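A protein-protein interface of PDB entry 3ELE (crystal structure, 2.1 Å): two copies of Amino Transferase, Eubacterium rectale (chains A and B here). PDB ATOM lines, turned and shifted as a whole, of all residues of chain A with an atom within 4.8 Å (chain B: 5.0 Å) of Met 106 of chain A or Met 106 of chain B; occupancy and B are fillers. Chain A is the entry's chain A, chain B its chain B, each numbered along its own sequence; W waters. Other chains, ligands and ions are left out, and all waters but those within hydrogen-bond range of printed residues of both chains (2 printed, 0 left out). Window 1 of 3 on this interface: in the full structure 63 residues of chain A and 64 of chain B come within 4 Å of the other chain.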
ATOM      1  N   MET A 104       5.769 -22.659 -10.965  1.00  0.00           N
ATOM      2  CA  MET A 104       5.011 -23.714 -10.288  1.00  0.00           C
ATOM      3  C   MET A 104       3.555 -23.701 -10.758  1.00  0.00           C
ATOM      4  O   MET A 104       2.921 -22.650 -10.781  1.00  0.00           O
ATOM      5  CB  MET A 104       5.084 -23.593  -8.762  1.00  0.00           C
ATOM      6  CG  MET A 104       6.522 -23.543  -8.191  1.00  0.00           C
ATOM      7  SD  MET A 104       7.675 -24.963  -8.791  1.00  0.00           S
ATOM      8  CE  MET A 104       6.753 -26.450  -7.966  1.00  0.00           C
ATOM      9  N   THR A 105       3.057 -24.883 -11.117  1.00  0.00           N
ATOM     10  CA  THR A 105       1.723 -25.051 -11.690  1.00  0.00           C
ATOM     11  C   THR A 105       0.887 -26.050 -10.897  1.00  0.00           C
ATOM     12  O   THR A 105       1.386 -26.736 -10.011  1.00  0.00           O
ATOM     13  CB  THR A 105       1.801 -25.527 -13.163  1.00  0.00           C
ATOM     14  OG1 THR A 105       2.400 -26.831 -13.209  1.00  0.00           O
ATOM     15  CG2 THR A 105       2.579 -24.539 -14.047  1.00  0.00           C
ATOM     16  N   MET A 106      -0.384 -26.127 -11.268  1.00  0.00           N
ATOM     17  CA  MET A 106      -1.360 -27.011 -10.665  1.00  0.00           C
ATOM     18  C   MET A 106      -1.506 -28.289 -11.483  1.00  0.00           C
ATOM     19  O   MET A 106      -2.599 -28.622 -11.955  1.00  0.00           O
ATOM     20  CB  MET A 106      -2.673 -26.244 -10.507  1.00  0.00           C
ATOM     21  CG  MET A 106      -2.453 -25.010  -9.584  1.00  0.00           C
ATOM     22  SD  MET A 106      -4.056 -24.165  -9.076  1.00  0.00           S
ATOM     23  CE  MET A 106      -4.459 -23.477 -10.749  1.00  0.00           C
ATOM     24  N   GLY A 107      -0.386 -29.000 -11.639  1.00  0.00           N
ATOM     25  CA  GLY A 107      -0.310 -30.240 -12.402  1.00  0.00           C
ATOM     26  C   GLY A 107       0.097 -30.038 -13.849  1.00  0.00           C
ATOM     27  O   GLY A 107       0.204 -28.903 -14.339  1.00  0.00           O
ATOM     28  N   ALA A 108       0.343 -31.172 -14.512  1.00  0.00           N
ATOM     29  CA  ALA A 108       0.759 -31.230 -15.900  1.00  0.00           C
ATOM     30  C   ALA A 108      -0.266 -30.662 -16.875  1.00  0.00           C
ATOM     31  O   ALA A 108       0.133 -30.088 -17.861  1.00  0.00           O
ATOM     32  CB  ALA A 108       1.122 -32.661 -16.295  1.00  0.00           C
ATOM     33  N   ALA A 110      -2.184 -28.144 -16.335  1.00  0.00           N
ATOM     34  CA  ALA A 110      -1.990 -26.703 -16.218  1.00  0.00           C
ATOM     35  C   ALA A 110      -0.695 -26.283 -16.949  1.00  0.00           C
ATOM     36  O   ALA A 110      -0.689 -25.284 -17.640  1.00  0.00           O
ATOM     37  CB  ALA A 110      -1.965 -26.278 -14.761  1.00  0.00           C
ATOM     38  N   ARG A 256      -2.536 -31.647  -7.455  1.00  0.00           N
ATOM     39  CA  ARG A 256      -2.330 -30.597  -8.468  1.00  0.00           C
ATOM     40  C   ARG A 256      -1.062 -29.777  -8.216  1.00  0.00           C
ATOM     41  O   ARG A 256      -1.121 -28.629  -7.785  1.00  0.00           O
ATOM     42  CB  ARG A 256      -3.589 -29.679  -8.582  1.00  0.00           C
ATOM     43  CG  ARG A 256      -4.951 -30.385  -8.543  1.00  0.00           C
ATOM     44  CD  ARG A 256      -5.013 -31.590  -9.453  1.00  0.00           C
ATOM     45  NE  ARG A 256      -4.794 -31.250 -10.848  1.00  0.00           N
ATOM     46  CZ  ARG A 256      -4.116 -31.954 -11.756  1.00  0.00           C
ATOM     47  NH1 ARG A 256      -3.428 -33.037 -11.453  1.00  0.00           N
ATOM     48  NH2 ARG A 256      -4.053 -31.486 -12.999  1.00  0.00           N
ATOM     49  N   ILE A 257       0.087 -30.400  -8.436  1.00  0.00           N
ATOM     50  CA  ILE A 257       1.378 -29.717  -8.262  1.00  0.00           C
ATOM     51  C   ILE A 257       2.380 -30.159  -9.329  1.00  0.00           C
ATOM     52  O   ILE A 257       2.669 -31.344  -9.497  1.00  0.00           O
ATOM     53  CB  ILE A 257       1.907 -29.891  -6.804  1.00  0.00           C
ATOM     54  CG1 ILE A 257       3.226 -29.126  -6.579  1.00  0.00           C
ATOM     55  CG2 ILE A 257       2.011 -31.393  -6.417  1.00  0.00           C
ATOM     56  CD1 ILE A 257       3.161 -27.640  -6.793  1.00  0.00           C
ATOM     57  N   GLY A 258       2.879 -29.189 -10.079  1.00  0.00           N
ATOM     58  CA  GLY A 258       3.871 -29.460 -11.082  1.00  0.00           C
ATOM     59  C   GLY A 258       4.590 -28.195 -11.464  1.00  0.00           C
ATOM     60  O   GLY A 258       4.619 -27.237 -10.691  1.00  0.00           O
ATOM     61  N   TYR A 285      -5.135 -18.910 -12.966  1.00  0.00           N
ATOM     62  CA  TYR A 285      -4.229 -19.485 -11.961  1.00  0.00           C
ATOM     63  C   TYR A 285      -3.642 -18.343 -11.154  1.00  0.00           C
ATOM     64  O   TYR A 285      -3.254 -17.332 -11.733  1.00  0.00           O
ATOM     65  CB  TYR A 285      -3.079 -20.302 -12.578  1.00  0.00           C
ATOM     66  CG  TYR A 285      -3.430 -21.344 -13.613  1.00  0.00           C
ATOM     67  CD1 TYR A 285      -4.618 -22.065 -13.559  1.00  0.00           C
ATOM     68  CD2 TYR A 285      -2.516 -21.690 -14.615  1.00  0.00           C
ATOM     69  CE1 TYR A 285      -4.908 -23.073 -14.516  1.00  0.00           C
ATOM     70  CE2 TYR A 285      -2.815 -22.703 -15.565  1.00  0.00           C
ATOM     71  CZ  TYR A 285      -4.030 -23.379 -15.490  1.00  0.00           C
ATOM     72  OH  TYR A 285      -4.410 -24.380 -16.356  1.00  0.00           O
ATOM     73  N   CYS A 287      -1.682 -19.206  -7.919  1.00  0.00           N
ATOM     74  CA  CYS A 287      -0.451 -19.892  -7.535  1.00  0.00           C
ATOM     75  C   CYS A 287      -0.730 -21.376  -7.304  1.00  0.00           C
ATOM     76  O   CYS A 287      -1.882 -21.743  -7.069  1.00  0.00           O
ATOM     77  CB  CYS A 287       0.155 -19.302  -6.255  1.00  0.00           C
ATOM     78  SG  CYS A 287      -0.800 -19.487  -4.721  1.00  0.00           S
ATOM     79  N   ALA A 288       0.320 -22.207  -7.348  1.00  0.00           N
ATOM     80  CA  ALA A 288       0.203 -23.632  -7.033  1.00  0.00           C
ATOM     81  C   ALA A 288      -0.128 -23.747  -5.558  1.00  0.00           C
ATOM     82  O   ALA A 288       0.213 -22.827  -4.796  1.00  0.00           O
ATOM     83  CB  ALA A 288       1.495 -24.377  -7.341  1.00  0.00           C
ATOM     84  N   PRO A 289      -0.789 -24.857  -5.132  1.00  0.00           N
ATOM     85  CA  PRO A 289      -1.138 -24.969  -3.721  1.00  0.00           C
ATOM     86  C   PRO A 289       0.081 -24.845  -2.778  1.00  0.00           C
ATOM     87  O   PRO A 289       1.046 -25.622  -2.867  1.00  0.00           O
ATOM     88  CB  PRO A 289      -1.817 -26.332  -3.633  1.00  0.00           C
ATOM     89  CG  PRO A 289      -2.340 -26.571  -4.988  1.00  0.00           C
ATOM     90  CD  PRO A 289      -1.273 -26.038  -5.874  1.00  0.00           C
ATOM     91  N   MET B 104     -16.532 -27.937  -7.909  1.00  0.00           N
ATOM     92  CA  MET B 104     -15.409 -27.497  -7.068  1.00  0.00           C
ATOM     93  C   MET B 104     -14.310 -26.969  -7.939  1.00  0.00           C
ATOM     94  O   MET B 104     -13.937 -27.603  -8.924  1.00  0.00           O
ATOM     95  CB  MET B 104     -14.894 -28.620  -6.184  1.00  0.00           C
ATOM     96  CG  MET B 104     -15.954 -29.283  -5.315  1.00  0.00           C
ATOM     97  SD  MET B 104     -16.952 -28.172  -4.166  1.00  0.00           S
ATOM     98  CE  MET B 104     -15.546 -27.568  -3.067  1.00  0.00           C
ATOM     99  N   THR B 105     -13.784 -25.814  -7.551  1.00  0.00           N
ATOM    100  CA  THR B 105     -12.774 -25.080  -8.306  1.00  0.00           C
ATOM    101  C   THR B 105     -11.533 -24.798  -7.477  1.00  0.00           C
ATOM    102  O   THR B 105     -11.534 -24.975  -6.261  1.00  0.00           O
ATOM    103  CB  THR B 105     -13.352 -23.724  -8.747  1.00  0.00           C
ATOM    104  OG1 THR B 105     -13.641 -22.946  -7.585  1.00  0.00           O
ATOM    105  CG2 THR B 105     -14.628 -23.915  -9.547  1.00  0.00           C
ATOM    106  N   MET B 106     -10.496 -24.295  -8.151  1.00  0.00           N
ATOM    107  CA  MET B 106      -9.243 -23.913  -7.523  1.00  0.00           C
ATOM    108  C   MET B 106      -9.201 -22.410  -7.239  1.00  0.00           C
ATOM    109  O   MET B 106      -8.410 -21.663  -7.805  1.00  0.00           O
ATOM    110  CB  MET B 106      -8.084 -24.391  -8.366  1.00  0.00           C
ATOM    111  CG  MET B 106      -8.143 -25.903  -8.532  1.00  0.00           C
ATOM    112  SD  MET B 106      -6.584 -26.621  -9.282  1.00  0.00           S
ATOM    113  CE  MET B 106      -6.677 -25.848 -10.755  1.00  0.00           C
ATOM    114  N   GLY B 107     -10.087 -21.983  -6.349  1.00  0.00           N
ATOM    115  CA  GLY B 107     -10.201 -20.584  -5.951  1.00  0.00           C
ATOM    116  C   GLY B 107     -11.246 -19.833  -6.734  1.00  0.00           C
ATOM    117  O   GLY B 107     -11.797 -20.350  -7.702  1.00  0.00           O
ATOM    118  N   ALA B 108     -11.542 -18.619  -6.279  1.00  0.00           N
ATOM    119  CA  ALA B 108     -12.538 -17.764  -6.916  1.00  0.00           C
ATOM    120  C   ALA B 108     -12.097 -17.262  -8.276  1.00  0.00           C
ATOM    121  O   ALA B 108     -12.965 -17.021  -9.106  1.00  0.00           O
ATOM    122  CB  ALA B 108     -12.959 -16.593  -6.006  1.00  0.00           C
ATOM    123  N   ALA B 110     -10.477 -19.054 -10.458  1.00  0.00           N
ATOM    124  CA  ALA B 110     -10.907 -20.173 -11.327  1.00  0.00           C
ATOM    125  C   ALA B 110     -12.416 -20.152 -11.544  1.00  0.00           C
ATOM    126  O   ALA B 110     -12.855 -20.287 -12.684  1.00  0.00           O
ATOM    127  CB  ALA B 110     -10.504 -21.517 -10.753  1.00  0.00           C
ATOM    128  N   ARG B 256      -6.047 -22.758  -2.813  1.00  0.00           N
ATOM    129  CA  ARG B 256      -6.782 -22.817  -4.066  1.00  0.00           C
ATOM    130  C   ARG B 256      -7.975 -23.778  -3.988  1.00  0.00           C
ATOM    131  O   ARG B 256      -7.942 -24.868  -4.578  1.00  0.00           O
ATOM    132  CB  ARG B 256      -5.831 -23.185  -5.238  1.00  0.00           C
ATOM    133  CG  ARG B 256      -4.452 -22.498  -5.260  1.00  0.00           C
ATOM    134  CD  ARG B 256      -4.534 -20.997  -4.989  1.00  0.00           C
ATOM    135  NE  ARG B 256      -5.465 -20.351  -5.912  1.00  0.00           N
ATOM    136  CZ  ARG B 256      -6.290 -19.334  -5.656  1.00  0.00           C
ATOM    137  NH1 ARG B 256      -6.422 -18.816  -4.447  1.00  0.00           N
ATOM    138  NH2 ARG B 256      -7.048 -18.859  -6.639  1.00  0.00           N
ATOM    139  N   ILE B 257      -8.998 -23.382  -3.224  1.00  0.00           N
ATOM    140  CA  ILE B 257     -10.226 -24.203  -3.049  1.00  0.00           C
ATOM    141  C   ILE B 257     -11.441 -23.285  -2.998  1.00  0.00           C
ATOM    142  O   ILE B 257     -11.502 -22.363  -2.190  1.00  0.00           O
ATOM    143  CB  ILE B 257     -10.123 -25.169  -1.819  1.00  0.00           C
ATOM    144  CG1 ILE B 257     -11.342 -26.108  -1.695  1.00  0.00           C
ATOM    145  CG2 ILE B 257      -9.894 -24.417  -0.509  1.00  0.00           C
ATOM    146  CD1 ILE B 257     -11.468 -27.178  -2.769  1.00  0.00           C
ATOM    147  N   GLY B 258     -12.381 -23.523  -3.903  1.00  0.00           N
ATOM    148  CA  GLY B 258     -13.623 -22.765  -3.981  1.00  0.00           C
ATOM    149  C   GLY B 258     -14.656 -23.545  -4.765  1.00  0.00           C
ATOM    150  O   GLY B 258     -14.506 -24.753  -4.943  1.00  0.00           O
ATOM    151  N   TYR B 285      -8.051 -27.360 -15.931  1.00  0.00           N
ATOM    152  CA  TYR B 285      -8.381 -27.875 -14.595  1.00  0.00           C
ATOM    153  C   TYR B 285      -8.788 -29.344 -14.738  1.00  0.00           C
ATOM    154  O   TYR B 285      -9.371 -29.741 -15.760  1.00  0.00           O
ATOM    155  CB  TYR B 285      -9.500 -27.079 -13.923  1.00  0.00           C
ATOM    156  CG  TYR B 285      -9.289 -25.564 -13.906  1.00  0.00           C
ATOM    157  CD1 TYR B 285      -8.146 -25.003 -13.369  1.00  0.00           C
ATOM    158  CD2 TYR B 285     -10.259 -24.700 -14.364  1.00  0.00           C
ATOM    159  CE1 TYR B 285      -7.971 -23.596 -13.312  1.00  0.00           C
ATOM    160  CE2 TYR B 285     -10.096 -23.304 -14.327  1.00  0.00           C
ATOM    161  CZ  TYR B 285      -8.947 -22.760 -13.826  1.00  0.00           C
ATOM    162  OH  TYR B 285      -8.791 -21.386 -13.794  1.00  0.00           O
ATOM    163  N   CYS B 287      -9.193 -31.337 -11.292  1.00  0.00           N
ATOM    164  CA  CYS B 287      -9.986 -31.365 -10.085  1.00  0.00           C
ATOM    165  C   CYS B 287      -9.402 -30.379  -9.087  1.00  0.00           C
ATOM    166  O   CYS B 287      -8.241 -29.971  -9.218  1.00  0.00           O
ATOM    167  CB  CYS B 287     -10.041 -32.752  -9.466  1.00  0.00           C
ATOM    168  SG  CYS B 287      -8.467 -33.478  -8.961  1.00  0.00           S
ATOM    169  N   ALA B 288     -10.223 -29.969  -8.121  1.00  0.00           N
ATOM    170  CA  ALA B 288      -9.740 -29.132  -7.031  1.00  0.00           C
ATOM    171  C   ALA B 288      -8.851 -30.056  -6.139  1.00  0.00           C
ATOM    172  O   ALA B 288      -9.069 -31.296  -6.112  1.00  0.00           O
ATOM    173  CB  ALA B 288     -10.919 -28.542  -6.243  1.00  0.00           C
ATOM    174  N   PRO B 289      -7.856 -29.480  -5.415  1.00  0.00           N
ATOM    175  CA  PRO B 289      -6.974 -30.286  -4.554  1.00  0.00           C
ATOM    176  C   PRO B 289      -7.706 -31.263  -3.583  1.00  0.00           C
ATOM    177  O   PRO B 289      -8.459 -30.831  -2.687  1.00  0.00           O
ATOM    178  CB  PRO B 289      -6.162 -29.233  -3.812  1.00  0.00           C
ATOM    179  CG  PRO B 289      -6.092 -28.096  -4.737  1.00  0.00           C
ATOM    180  CD  PRO B 289      -7.467 -28.053  -5.359  1.00  0.00           C
HETATM  181  O   HOH W   1      -6.938 -29.215 -11.537  1.00  0.00           O
HETATM  182  O   HOH W   2      -4.285 -20.957  -8.684  1.00  0.00           O
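The side-chain sulfur (SD) of Met 106 of chain B sits close to the side-chain sulfur (SD) of Met 106 of chain A (3.5 Å).
O of Met 106 of chain B is in hydrogen-bond range of NH2 of Arg 256 of chain B (3.3 Å).
O of Met 106 of chain A lies within hydrogen-bond range of NH2 of Arg 256 of chain A (3.4 Å).
Among the printed residues, pairs that only touch across the chains: Arg 256 of chain A with Cys 287 of chain B (3.4 Å), Tyr 285 of chain A with Tyr 285 of chain B (3.3 Å) and Cys 287 of chain A with Arg 256 of chain B (3.2 Å).
Of chain B, only Met 106 comes within 4 Å of Met 106 of chain A.
Of the printed residues of chain B, Arg 256 of chain A touches Cys 287.
Printed residues of chain B within 4 Å of Tyr 285 of chain A: Tyr 285.
Of the printed residues of chain B, Cys 287 of chain A touches Arg 256.
Of chain A, only Met 106 comes within 4 Å of Met 106 of chain B.
Of the printed residues of chain A, Cys 287 of chain B touches Arg 256 (3.4 Å).
Pro 289 of chain B touches none of the printed residues of chain A.
The nearest residue of chain B that does not touch Met 106 of chain A is Arg 256 of chain B (4.2 Å).
The nearest residue of chain A that does not touch Met 106 of chain B is Arg 256 of chain A (4.2 Å).
Of the 13 printed residues of chain A, 4 touch a printed residue of chain B.
Hydrophobic or aromatic side chains of chain A that line the printed part of chain B: Met 106 and Tyr 285.
Printed residues of chain B that touch a printed residue of chain A: Met 106, Arg 256, Tyr 285 and Cys 287.
Hydrophobic or aromatic side chains of chain B within 4 Å of the printed part of chain A: Met 106 and Tyr 285.
Met 106 of chain B touches its own counterpart, Met 106 of chain A.
Arg 256 of chain A touches Cys 287 of chain B, and with the chains exchanged Cys 287 of chain A touches Arg 256 of chain B.
Tyr 285 of chain B touches its own counterpart, Tyr 285 of chain A.
Positions printed for both chains: 104, 105, 106, 107, 108, 110, 256, 257, 258, 285, 287, 288 and 289.
Of the 4 pairs that touch across the chains among the printed residues, 4 have their exchanged pair printed and touching as well.
Water W1 lies within hydrogen-bond range of the backbone carbonyl oxygen of Cys 287 of chain B (2.8 Å), the guanidinium group of Arg 256 of chain A (3.0 Å) and the side-chain sulfur of Met 106 of chain B (3.5 Å).
Water W2 lies within hydrogen-bond range of the backbone carbonyl oxygen of Cys 287 of chain A, the guanidinium group of Arg 256 of chain B and the side-chain sulfur of Met 106 of chain A.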
